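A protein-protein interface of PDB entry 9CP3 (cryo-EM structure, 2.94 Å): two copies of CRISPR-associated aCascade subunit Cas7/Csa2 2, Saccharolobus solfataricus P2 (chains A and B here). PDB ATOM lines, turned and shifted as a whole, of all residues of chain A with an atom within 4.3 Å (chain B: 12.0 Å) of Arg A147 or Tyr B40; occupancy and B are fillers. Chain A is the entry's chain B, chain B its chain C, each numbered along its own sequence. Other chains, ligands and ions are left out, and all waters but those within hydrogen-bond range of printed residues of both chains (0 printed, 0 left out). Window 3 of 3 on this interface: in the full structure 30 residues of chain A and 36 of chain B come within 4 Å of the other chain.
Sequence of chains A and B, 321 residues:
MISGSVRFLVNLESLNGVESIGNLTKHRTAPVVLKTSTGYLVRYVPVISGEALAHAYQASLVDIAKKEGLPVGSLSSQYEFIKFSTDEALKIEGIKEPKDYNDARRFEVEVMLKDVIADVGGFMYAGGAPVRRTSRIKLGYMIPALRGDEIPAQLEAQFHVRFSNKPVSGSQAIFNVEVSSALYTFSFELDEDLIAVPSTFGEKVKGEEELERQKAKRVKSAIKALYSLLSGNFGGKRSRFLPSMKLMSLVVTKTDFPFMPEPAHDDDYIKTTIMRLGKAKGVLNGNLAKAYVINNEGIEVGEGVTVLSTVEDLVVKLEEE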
ATOM      1  N   LEU A   9      -0.341   7.770  -5.807  1.00  0.00           N
ATOM      2  CA  LEU A   9      -0.015   6.373  -6.080  1.00  0.00           C
ATOM      3  C   LEU A   9       0.552   6.309  -7.491  1.00  0.00           C
ATOM      4  O   LEU A   9      -0.175   6.547  -8.463  1.00  0.00           O
ATOM      5  CB  LEU A   9      -1.249   5.482  -5.937  1.00  0.00           C
ATOM      6  CG  LEU A   9      -1.023   3.971  -5.915  1.00  0.00           C
ATOM      7  CD1 LEU A   9      -0.581   3.518  -4.538  1.00  0.00           C
ATOM      8  CD2 LEU A   9      -2.287   3.240  -6.336  1.00  0.00           C
ATOM      9  N   ALA A 145       5.565   6.653   1.718  1.00  0.00           N
ATOM     10  CA  ALA A 145       5.065   6.740   3.084  1.00  0.00           C
ATOM     11  C   ALA A 145       5.791   5.753   3.989  1.00  0.00           C
ATOM     12  O   ALA A 145       5.890   4.563   3.681  1.00  0.00           O
ATOM     13  CB  ALA A 145       3.561   6.471   3.108  1.00  0.00           C
ATOM     14  N   LEU A 146       6.298   6.259   5.114  1.00  0.00           N
ATOM     15  CA  LEU A 146       6.965   5.426   6.115  1.00  0.00           C
ATOM     16  C   LEU A 146       5.932   4.950   7.138  1.00  0.00           C
ATOM     17  O   LEU A 146       5.877   5.399   8.284  1.00  0.00           O
ATOM     18  CB  LEU A 146       8.100   6.196   6.777  1.00  0.00           C
ATOM     19  CG  LEU A 146       9.067   6.928   5.845  1.00  0.00           C
ATOM     20  CD1 LEU A 146      10.199   7.554   6.637  1.00  0.00           C
ATOM     21  CD2 LEU A 146       9.618   5.980   4.794  1.00  0.00           C
ATOM     22  N   ARG A 147       5.102   4.015   6.692  1.00  0.00           N
ATOM     23  CA  ARG A 147       3.979   3.523   7.475  1.00  0.00           C
ATOM     24  C   ARG A 147       4.183   2.056   7.823  1.00  0.00           C
ATOM     25  O   ARG A 147       4.626   1.264   6.985  1.00  0.00           O
ATOM     26  CB  ARG A 147       2.671   3.686   6.703  1.00  0.00           C
ATOM     27  CG  ARG A 147       1.429   3.331   7.494  1.00  0.00           C
ATOM     28  CD  ARG A 147       0.183   3.588   6.670  1.00  0.00           C
ATOM     29  NE  ARG A 147       0.417   3.332   5.255  1.00  0.00           N
ATOM     30  CZ  ARG A 147       0.451   2.124   4.709  1.00  0.00           C
ATOM     31  NH1 ARG A 147       0.251   1.034   5.432  1.00  0.00           N
ATOM     32  NH2 ARG A 147       0.696   2.006   3.408  1.00  0.00           N
ATOM     33  N   GLY A 148       3.847   1.698   9.061  1.00  0.00           N
ATOM     34  CA  GLY A 148       3.963   0.312   9.480  1.00  0.00           C
ATOM     35  C   GLY A 148       5.408  -0.147   9.504  1.00  0.00           C
ATOM     36  O   GLY A 148       6.326   0.610   9.837  1.00  0.00           O
ATOM     37  N   ASP A 149       5.614  -1.415   9.141  1.00  0.00           N
ATOM     38  CA  ASP A 149       6.942  -2.011   9.117  1.00  0.00           C
ATOM     39  C   ASP A 149       7.469  -2.277   7.716  1.00  0.00           C
ATOM     40  O   ASP A 149       8.686  -2.406   7.549  1.00  0.00           O
ATOM     41  CB  ASP A 149       6.950  -3.328   9.906  1.00  0.00           C
ATOM     42  CG  ASP A 149       6.755  -3.116  11.393  1.00  0.00           C
ATOM     43  OD1 ASP A 149       6.501  -1.964  11.803  1.00  0.00           O
ATOM     44  OD2 ASP A 149       6.856  -4.101  12.155  1.00  0.00           O
ATOM     45  N   GLU A 150       6.598  -2.360   6.715  1.00  0.00           N
ATOM     46  CA  GLU A 150       6.997  -2.633   5.341  1.00  0.00           C
ATOM     47  C   GLU A 150       6.742  -1.408   4.476  1.00  0.00           C
ATOM     48  O   GLU A 150       5.626  -0.875   4.459  1.00  0.00           O
ATOM     49  CB  GLU A 150       6.232  -3.835   4.784  1.00  0.00           C
ATOM     50  CG  GLU A 150       6.185  -5.028   5.721  1.00  0.00           C
ATOM     51  CD  GLU A 150       5.466  -6.217   5.115  1.00  0.00           C
ATOM     52  OE1 GLU A 150       4.932  -6.085   3.994  1.00  0.00           O
ATOM     53  OE2 GLU A 150       5.433  -7.287   5.761  1.00  0.00           O
ATOM     54  N   PRO A 152       5.868   0.396   1.182  1.00  0.00           N
ATOM     55  CA  PRO A 152       5.181   0.009  -0.068  1.00  0.00           C
ATOM     56  C   PRO A 152       5.831   0.630  -1.299  1.00  0.00           C
ATOM     57  O   PRO A 152       5.263   1.476  -1.996  1.00  0.00           O
ATOM     58  CB  PRO A 152       3.755   0.516   0.175  1.00  0.00           C
ATOM     59  CG  PRO A 152       3.931   1.708   1.057  1.00  0.00           C
ATOM     60  CD  PRO A 152       5.188   1.507   1.869  1.00  0.00           C
ATOM     61  N   LEU A 183       4.066   4.661  -3.296  1.00  0.00           N
ATOM     62  CA  LEU A 183       2.986   5.486  -2.760  1.00  0.00           C
ATOM     63  C   LEU A 183       3.652   6.741  -2.201  1.00  0.00           C
ATOM     64  O   LEU A 183       4.076   6.779  -1.046  1.00  0.00           O
ATOM     65  CB  LEU A 183       2.190   4.737  -1.695  1.00  0.00           C
ATOM     66  CG  LEU A 183       1.210   5.539  -0.833  1.00  0.00           C
ATOM     67  CD1 LEU A 183      -0.029   5.919  -1.624  1.00  0.00           C
ATOM     68  CD2 LEU A 183       0.838   4.763   0.419  1.00  0.00           C
ATOM     69  N   MET A 248      -5.217  10.089  -3.785  1.00  0.00           N
ATOM     70  CA  MET A 248      -5.742   9.310  -2.670  1.00  0.00           C
ATOM     71  C   MET A 248      -6.262  10.184  -1.541  1.00  0.00           C
ATOM     72  O   MET A 248      -7.397   9.989  -1.087  1.00  0.00           O
ATOM     73  CB  MET A 248      -4.662   8.354  -2.137  1.00  0.00           C
ATOM     74  CG  MET A 248      -3.970   7.530  -3.209  1.00  0.00           C
ATOM     75  SD  MET A 248      -5.094   6.450  -4.115  1.00  0.00           S
ATOM     76  CE  MET A 248      -5.955   5.634  -2.773  1.00  0.00           C
ATOM     77  N   HIS A 265       2.378  10.407   6.456  1.00  0.00           N
ATOM     78  CA  HIS A 265       2.984   9.113   6.754  1.00  0.00           C
ATOM     79  C   HIS A 265       1.987   8.161   7.401  1.00  0.00           C
ATOM     80  O   HIS A 265       1.950   6.971   7.068  1.00  0.00           O
ATOM     81  CB  HIS A 265       4.203   9.304   7.652  1.00  0.00           C
ATOM     82  CG  HIS A 265       5.354   9.969   6.969  1.00  0.00           C
ATOM     83  ND1 HIS A 265       6.546  10.235   7.606  1.00  0.00           N
ATOM     84  CD2 HIS A 265       5.496  10.421   5.701  1.00  0.00           C
ATOM     85  CE1 HIS A 265       7.372  10.823   6.761  1.00  0.00           C
ATOM     86  NE2 HIS A 265       6.760  10.948   5.597  1.00  0.00           N
ATOM     87  N   ASP A 267      -1.975   6.917   8.766  1.00  0.00           N
ATOM     88  CA  ASP A 267      -3.350   6.923   8.277  1.00  0.00           C
ATOM     89  C   ASP A 267      -4.182   8.006   8.946  1.00  0.00           C
ATOM     90  O   ASP A 267      -5.159   8.484   8.358  1.00  0.00           O
ATOM     91  CB  ASP A 267      -4.000   5.558   8.504  1.00  0.00           C
ATOM     92  CG  ASP A 267      -3.209   4.426   7.888  1.00  0.00           C
ATOM     93  OD1 ASP A 267      -2.306   3.898   8.568  1.00  0.00           O
ATOM     94  OD2 ASP A 267      -3.488   4.067   6.725  1.00  0.00           O
ATOM     95  N   GLU A 297      -9.568   7.301  -0.263  1.00  0.00           N
ATOM     96  CA  GLU A 297      -9.173   6.017   0.297  1.00  0.00           C
ATOM     97  C   GLU A 297      -9.969   5.632   1.538  1.00  0.00           C
ATOM     98  O   GLU A 297      -9.671   4.603   2.152  1.00  0.00           O
ATOM     99  CB  GLU A 297      -7.674   6.025   0.614  1.00  0.00           C
ATOM    100  CG  GLU A 297      -7.262   7.031   1.671  1.00  0.00           C
ATOM    101  CD  GLU A 297      -5.763   7.060   1.890  1.00  0.00           C
ATOM    102  OE1 GLU A 297      -5.047   6.307   1.199  1.00  0.00           O
ATOM    103  OE2 GLU A 297      -5.298   7.835   2.751  1.00  0.00           O
ATOM    104  N   PRO B  31       7.062  -4.789 -10.983  1.00  0.00           N
ATOM    105  CA  PRO B  31       6.339  -4.686  -9.714  1.00  0.00           C
ATOM    106  C   PRO B  31       5.313  -3.564  -9.727  1.00  0.00           C
ATOM    107  O   PRO B  31       5.451  -2.556 -10.421  1.00  0.00           O
ATOM    108  CB  PRO B  31       7.453  -4.382  -8.698  1.00  0.00           C
ATOM    109  CG  PRO B  31       8.754  -4.456  -9.464  1.00  0.00           C
ATOM    110  CD  PRO B  31       8.410  -4.210 -10.886  1.00  0.00           C
ATOM    111  N   VAL B  32       4.271  -3.756  -8.923  1.00  0.00           N
ATOM    112  CA  VAL B  32       3.203  -2.777  -8.766  1.00  0.00           C
ATOM    113  C   VAL B  32       2.814  -2.698  -7.297  1.00  0.00           C
ATOM    114  O   VAL B  32       2.882  -3.687  -6.559  1.00  0.00           O
ATOM    115  CB  VAL B  32       1.967  -3.111  -9.633  1.00  0.00           C
ATOM    116  CG1 VAL B  32       2.273  -2.908 -11.106  1.00  0.00           C
ATOM    117  CG2 VAL B  32       1.500  -4.529  -9.372  1.00  0.00           C
ATOM    118  N   VAL B  33       2.409  -1.505  -6.874  1.00  0.00           N
ATOM    119  CA  VAL B  33       1.921  -1.266  -5.521  1.00  0.00           C
ATOM    120  C   VAL B  33       0.408  -1.131  -5.597  1.00  0.00           C
ATOM    121  O   VAL B  33      -0.112  -0.252  -6.295  1.00  0.00           O
ATOM    122  CB  VAL B  33       2.557  -0.009  -4.908  1.00  0.00           C
ATOM    123  CG1 VAL B  33       1.925   0.304  -3.567  1.00  0.00           C
ATOM    124  CG2 VAL B  33       4.059  -0.185  -4.774  1.00  0.00           C
ATOM    125  N   LEU B  34      -0.302  -1.998  -4.881  1.00  0.00           N
ATOM    126  CA  LEU B  34      -1.751  -2.080  -4.982  1.00  0.00           C
ATOM    127  C   LEU B  34      -2.374  -1.927  -3.602  1.00  0.00           C
ATOM    128  O   LEU B  34      -1.832  -2.415  -2.605  1.00  0.00           O
ATOM    129  CB  LEU B  34      -2.174  -3.411  -5.626  1.00  0.00           C
ATOM    130  CG  LEU B  34      -3.629  -3.604  -6.060  1.00  0.00           C
ATOM    131  CD1 LEU B  34      -3.691  -4.553  -7.242  1.00  0.00           C
ATOM    132  CD2 LEU B  34      -4.489  -4.135  -4.935  1.00  0.00           C
ATOM    133  N   LYS B  35      -3.519  -1.253  -3.552  1.00  0.00           N
ATOM    134  CA  LYS B  35      -4.207  -0.959  -2.303  1.00  0.00           C
ATOM    135  C   LYS B  35      -5.355  -1.942  -2.113  1.00  0.00           C
ATOM    136  O   LYS B  35      -6.241  -2.041  -2.968  1.00  0.00           O
ATOM    137  CB  LYS B  35      -4.725   0.480  -2.303  1.00  0.00           C
ATOM    138  CG  LYS B  35      -5.112   1.014  -0.934  1.00  0.00           C
ATOM    139  CD  LYS B  35      -6.612   0.916  -0.713  1.00  0.00           C
ATOM    140  CE  LYS B  35      -7.023   1.562   0.599  1.00  0.00           C
ATOM    141  NZ  LYS B  35      -8.491   1.459   0.820  1.00  0.00           N
ATOM    142  N   THR B  36      -5.339  -2.661  -0.995  1.00  0.00           N
ATOM    143  CA  THR B  36      -6.407  -3.573  -0.617  1.00  0.00           C
ATOM    144  C   THR B  36      -7.008  -3.133   0.711  1.00  0.00           C
ATOM    145  O   THR B  36      -6.502  -2.230   1.383  1.00  0.00           O
ATOM    146  CB  THR B  36      -5.903  -5.018  -0.501  1.00  0.00           C
ATOM    147  OG1 THR B  36      -4.824  -5.076   0.438  1.00  0.00           O
ATOM    148  CG2 THR B  36      -5.432  -5.536  -1.842  1.00  0.00           C
ATOM    149  N   SER B  37      -8.094  -3.807   1.095  1.00  0.00           N
ATOM    150  CA  SER B  37      -8.760  -3.497   2.353  1.00  0.00           C
ATOM    151  C   SER B  37      -7.854  -3.718   3.556  1.00  0.00           C
ATOM    152  O   SER B  37      -8.115  -3.159   4.626  1.00  0.00           O
ATOM    153  CB  SER B  37     -10.026  -4.342   2.498  1.00  0.00           C
ATOM    154  OG  SER B  37      -9.707  -5.673   2.862  1.00  0.00           O
ATOM    155  N   THR B  38      -6.800  -4.515   3.408  1.00  0.00           N
ATOM    156  CA  THR B  38      -5.852  -4.764   4.484  1.00  0.00           C
ATOM    157  C   THR B  38      -4.644  -3.836   4.441  1.00  0.00           C
ATOM    158  O   THR B  38      -3.740  -3.986   5.269  1.00  0.00           O
ATOM    159  CB  THR B  38      -5.377  -6.220   4.446  1.00  0.00           C
ATOM    160  OG1 THR B  38      -4.698  -6.470   3.209  1.00  0.00           O
ATOM    161  CG2 THR B  38      -6.562  -7.166   4.562  1.00  0.00           C
ATOM    162  N   GLY B  39      -4.599  -2.896   3.500  1.00  0.00           N
ATOM    163  CA  GLY B  39      -3.486  -1.969   3.439  1.00  0.00           C
ATOM    164  C   GLY B  39      -2.879  -1.822   2.060  1.00  0.00           C
ATOM    165  O   GLY B  39      -3.598  -1.645   1.073  1.00  0.00           O
ATOM    166  N   TYR B  40      -1.553  -1.889   1.976  1.00  0.00           N
ATOM    167  CA  TYR B  40      -0.843  -1.739   0.715  1.00  0.00           C
ATOM    168  C   TYR B  40       0.082  -2.929   0.516  1.00  0.00           C
ATOM    169  O   TYR B  40       0.757  -3.364   1.453  1.00  0.00           O
ATOM    170  CB  TYR B  40      -0.039  -0.434   0.689  1.00  0.00           C
ATOM    171  CG  TYR B  40      -0.888   0.800   0.488  1.00  0.00           C
ATOM    172  CD1 TYR B  40      -1.710   1.272   1.503  1.00  0.00           C
ATOM    173  CD2 TYR B  40      -0.872   1.492  -0.714  1.00  0.00           C
ATOM    174  CE1 TYR B  40      -2.488   2.398   1.328  1.00  0.00           C
ATOM    175  CE2 TYR B  40      -1.650   2.619  -0.899  1.00  0.00           C
ATOM    176  CZ  TYR B  40      -2.455   3.066   0.126  1.00  0.00           C
ATOM    177  OH  TYR B  40      -3.229   4.187  -0.051  1.00  0.00           O
ATOM    178  N   LEU B  41       0.116  -3.452  -0.709  1.00  0.00           N
ATOM    179  CA  LEU B  41       0.904  -4.631  -1.028  1.00  0.00           C
ATOM    180  C   LEU B  41       1.720  -4.386  -2.290  1.00  0.00           C
ATOM    181  O   LEU B  41       1.419  -3.494  -3.087  1.00  0.00           O
ATOM    182  CB  LEU B  41       0.018  -5.869  -1.221  1.00  0.00           C
ATOM    183  CG  LEU B  41      -0.423  -6.633   0.029  1.00  0.00           C
ATOM    184  CD1 LEU B  41      -1.601  -5.949   0.701  1.00  0.00           C
ATOM    185  CD2 LEU B  41      -0.767  -8.069  -0.323  1.00  0.00           C
ATOM    186  N   VAL B  42       2.764  -5.192  -2.457  1.00  0.00           N
ATOM    187  CA  VAL B  42       3.632  -5.147  -3.627  1.00  0.00           C
ATOM    188  C   VAL B  42       3.514  -6.484  -4.345  1.00  0.00           C
ATOM    189  O   VAL B  42       3.692  -7.541  -3.728  1.00  0.00           O
ATOM    190  CB  VAL B  42       5.093  -4.855  -3.245  1.00  0.00           C
ATOM    191  CG1 VAL B  42       5.931  -4.636  -4.489  1.00  0.00           C
ATOM    192  CG2 VAL B  42       5.167  -3.642  -2.335  1.00  0.00           C
ATOM    193  N   ARG B  43       3.222  -6.438  -5.641  1.00  0.00           N
ATOM    194  CA  ARG B  43       3.018  -7.641  -6.435  1.00  0.00           C
ATOM    195  C   ARG B  43       3.817  -7.552  -7.727  1.00  0.00           C
ATOM    196  O   ARG B  43       4.359  -6.503  -8.079  1.00  0.00           O
ATOM    197  CB  ARG B  43       1.533  -7.861  -6.745  1.00  0.00           C
ATOM    198  CG  ARG B  43       0.702  -8.249  -5.540  1.00  0.00           C
ATOM    199  CD  ARG B  43       0.913  -9.711  -5.190  1.00  0.00           C
ATOM    200  NE  ARG B  43       0.324 -10.062  -3.904  1.00  0.00           N
ATOM    201  CZ  ARG B  43      -0.972 -10.246  -3.696  1.00  0.00           C
ATOM    202  NH1 ARG B  43      -1.854 -10.128  -4.676  1.00  0.00           N
ATOM    203  NH2 ARG B  43      -1.396 -10.559  -2.476  1.00  0.00           N
ATOM    204  N   TYR B  44       3.884  -8.676  -8.437  1.00  0.00           N
ATOM    205  CA  TYR B  44       4.597  -8.777  -9.703  1.00  0.00           C
ATOM    206  C   TYR B  44       3.607  -9.143 -10.796  1.00  0.00           C
ATOM    207  O   TYR B  44       2.858 -10.115 -10.656  1.00  0.00           O
ATOM    208  CB  TYR B  44       5.707  -9.825  -9.624  1.00  0.00           C
ATOM    209  CG  TYR B  44       6.999  -9.299  -9.058  1.00  0.00           C
ATOM    210  CD1 TYR B  44       7.214  -9.264  -7.689  1.00  0.00           C
ATOM    211  CD2 TYR B  44       8.005  -8.838  -9.890  1.00  0.00           C
ATOM    212  CE1 TYR B  44       8.395  -8.784  -7.164  1.00  0.00           C
ATOM    213  CE2 TYR B  44       9.189  -8.357  -9.377  1.00  0.00           C
ATOM    214  CZ  TYR B  44       9.379  -8.332  -8.014  1.00  0.00           C
ATOM    215  OH  TYR B  44      10.560  -7.851  -7.498  1.00  0.00           O
ATOM    216  N   LEU B 146      -5.072  -2.389 -11.891  1.00  0.00           N
ATOM    217  CA  LEU B 146      -4.914  -2.610 -10.453  1.00  0.00           C
ATOM    218  C   LEU B 146      -6.231  -2.267  -9.755  1.00  0.00           C
ATOM    219  O   LEU B 146      -6.377  -1.254  -9.072  1.00  0.00           O
ATOM    220  CB  LEU B 146      -3.751  -1.791  -9.910  1.00  0.00           C
ATOM    221  CG  LEU B 146      -2.440  -1.874 -10.692  1.00  0.00           C
ATOM    222  CD1 LEU B 146      -1.347  -1.104  -9.978  1.00  0.00           C
ATOM    223  CD2 LEU B 146      -2.025  -3.320 -10.894  1.00  0.00           C
ATOM    224  N   GLY B 148      -9.600  -3.520  -7.357  1.00  0.00           N
ATOM    225  CA  GLY B 148     -10.020  -4.425  -6.301  1.00  0.00           C
ATOM    226  C   GLY B 148      -8.837  -4.990  -5.538  1.00  0.00           C
ATOM    227  O   GLY B 148      -7.826  -4.314  -5.316  1.00  0.00           O
ATOM    228  N   ASP B 149      -8.963  -6.253  -5.128  1.00  0.00           N
ATOM    229  CA  ASP B 149      -7.917  -6.927  -4.375  1.00  0.00           C
ATOM    230  C   ASP B 149      -7.188  -8.005  -5.163  1.00  0.00           C
ATOM    231  O   ASP B 149      -6.068  -8.367  -4.788  1.00  0.00           O
ATOM    232  CB  ASP B 149      -8.499  -7.558  -3.102  1.00  0.00           C
ATOM    233  CG  ASP B 149      -8.959  -6.523  -2.095  1.00  0.00           C
ATOM    234  OD1 ASP B 149      -8.933  -5.319  -2.426  1.00  0.00           O
ATOM    235  OD2 ASP B 149      -9.345  -6.911  -0.973  1.00  0.00           O
ATOM    236  N   GLU B 150      -7.783  -8.522  -6.233  1.00  0.00           N
ATOM    237  CA  GLU B 150      -7.178  -9.570  -7.043  1.00  0.00           C
ATOM    238  C   GLU B 150      -6.839  -9.016  -8.419  1.00  0.00           C
ATOM    239  O   GLU B 150      -7.703  -8.449  -9.095  1.00  0.00           O
ATOM    240  CB  GLU B 150      -8.118 -10.769  -7.172  1.00  0.00           C
ATOM    241  CG  GLU B 150      -8.741 -11.205  -5.857  1.00  0.00           C
ATOM    242  CD  GLU B 150      -9.624 -12.427  -6.007  1.00  0.00           C
ATOM    243  OE1 GLU B 150      -9.817 -12.885  -7.153  1.00  0.00           O
ATOM    244  OE2 GLU B 150     -10.124 -12.930  -4.979  1.00  0.00           O
ATOM    245  N   ILE B 151      -5.588  -9.184  -8.826  1.00  0.00           N
ATOM    246  CA  ILE B 151      -5.148  -8.710 -10.140  1.00  0.00           C
ATOM    247  C   ILE B 151      -5.611  -9.704 -11.201  1.00  0.00           C
ATOM    248  O   ILE B 151      -5.310 -10.902 -11.088  1.00  0.00           O
ATOM    249  CB  ILE B 151      -3.634  -8.545 -10.169  1.00  0.00           C
ATOM    250  CG1 ILE B 151      -3.161  -7.778  -8.935  1.00  0.00           C
ATOM    251  CG2 ILE B 151      -3.207  -7.831 -11.436  1.00  0.00           C
ATOM    252  CD1 ILE B 151      -1.664  -7.781  -8.753  1.00  0.00           C
ATOM    253  N   HIS B 265      -7.796   2.331 -14.293  1.00  0.00           N
ATOM    254  CA  HIS B 265      -7.711   1.369 -13.201  1.00  0.00           C
ATOM    255  C   HIS B 265      -9.082   1.087 -12.600  1.00  0.00           C
ATOM    256  O   HIS B 265      -9.410  -0.067 -12.301  1.00  0.00           O
ATOM    257  CB  HIS B 265      -6.747   1.869 -12.128  1.00  0.00           C
ATOM    258  CG  HIS B 265      -5.315   1.874 -12.559  1.00  0.00           C
ATOM    259  ND1 HIS B 265      -4.292   2.293 -11.736  1.00  0.00           N
ATOM    260  CD2 HIS B 265      -4.735   1.510 -13.726  1.00  0.00           C
ATOM    261  CE1 HIS B 265      -3.142   2.186 -12.378  1.00  0.00           C
ATOM    262  NE2 HIS B 265      -3.383   1.714 -13.588  1.00  0.00           N
ATOM    263  N   ASP B 266      -9.894   2.121 -12.417  1.00  0.00           N
ATOM    264  CA  ASP B 266     -11.192   1.997 -11.777  1.00  0.00           C
ATOM    265  C   ASP B 266     -12.301   1.941 -12.818  1.00  0.00           C
ATOM    266  O   ASP B 266     -12.149   2.405 -13.951  1.00  0.00           O
ATOM    267  CB  ASP B 266     -11.434   3.165 -10.819  1.00  0.00           C
ATOM    268  CG  ASP B 266     -10.551   3.103  -9.592  1.00  0.00           C
ATOM    269  OD1 ASP B 266     -10.241   1.983  -9.137  1.00  0.00           O
ATOM    270  OD2 ASP B 266     -10.163   4.175  -9.083  1.00  0.00           O
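Positions printed for both chains: 146, 148, 149, 150 and 265.
Of chain B, only Tyr B40 (3.2 Å) comes within 4 Å of Arg A147. Printed residues of chain A within 4 Å of Tyr B40: Leu A9 (3.9 Å), Arg A147 (3.2 Å), Pro A152 (3.9 Å), Leu A183 (3.5 Å) and Glu A297 (3.1 Å). No residue of chain B comes within 4 Å of Ala A145. No residue of chain B comes within 4 Å of Leu A146. Pro A152 touches just these residues of chain B: Val B33 and Tyr B40. Of chain B, only Tyr B40 (3.5 Å) comes within 4 Å of Leu A183. No residue of chain B comes within 4 Å of Asp A267. Of the printed residues of chain B, Glu A297 touches Lys B35 (3.6 Å) and Tyr B40 (3.1 Å). Of the printed residues of chain B, Leu A9 touches Tyr B40 (3.9 Å). Printed residues of chain A within 4 Å of Lys B35: Glu A297. Of the printed residues of chain A, Val B33 touches Pro A152. Thr B38 touches none of the printed residues of chain A. The nearest residue of chain B that does not touch Arg A147 is Gly B39 (5.2 Å).
OE1 of Glu A297 is in hydrogen-bond range of OH of Tyr B40 (3.1 Å).
N of Ala A145 lies within hydrogen-bond range of O of Leu A183 (3.1 Å).
Of the 13 printed residues of chain A, 5 touch a printed residue of chain B. Hydrophobic or aromatic side chains of chain A that line the printed part of chain B: Leu A9, Pro A152 and Leu A183. Along chain A the printed residues that touch a printed residue of chain B span positions 9 to 297. Of the 21 printed residues of chain B, 3 touch a printed residue of chain A.
Among the printed residues, merely in contact across the chains: Arg A147 with Tyr B40 (3.2 Å), Pro A152 with Val B33 (3.5 Å), Leu A183 with Tyr B40 (3.5 Å), Glu A297 with Lys B35 (3.6 Å), Leu A9 with Tyr B40 (3.9 Å) and Pro A152 with Tyr B40 (3.9 Å).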
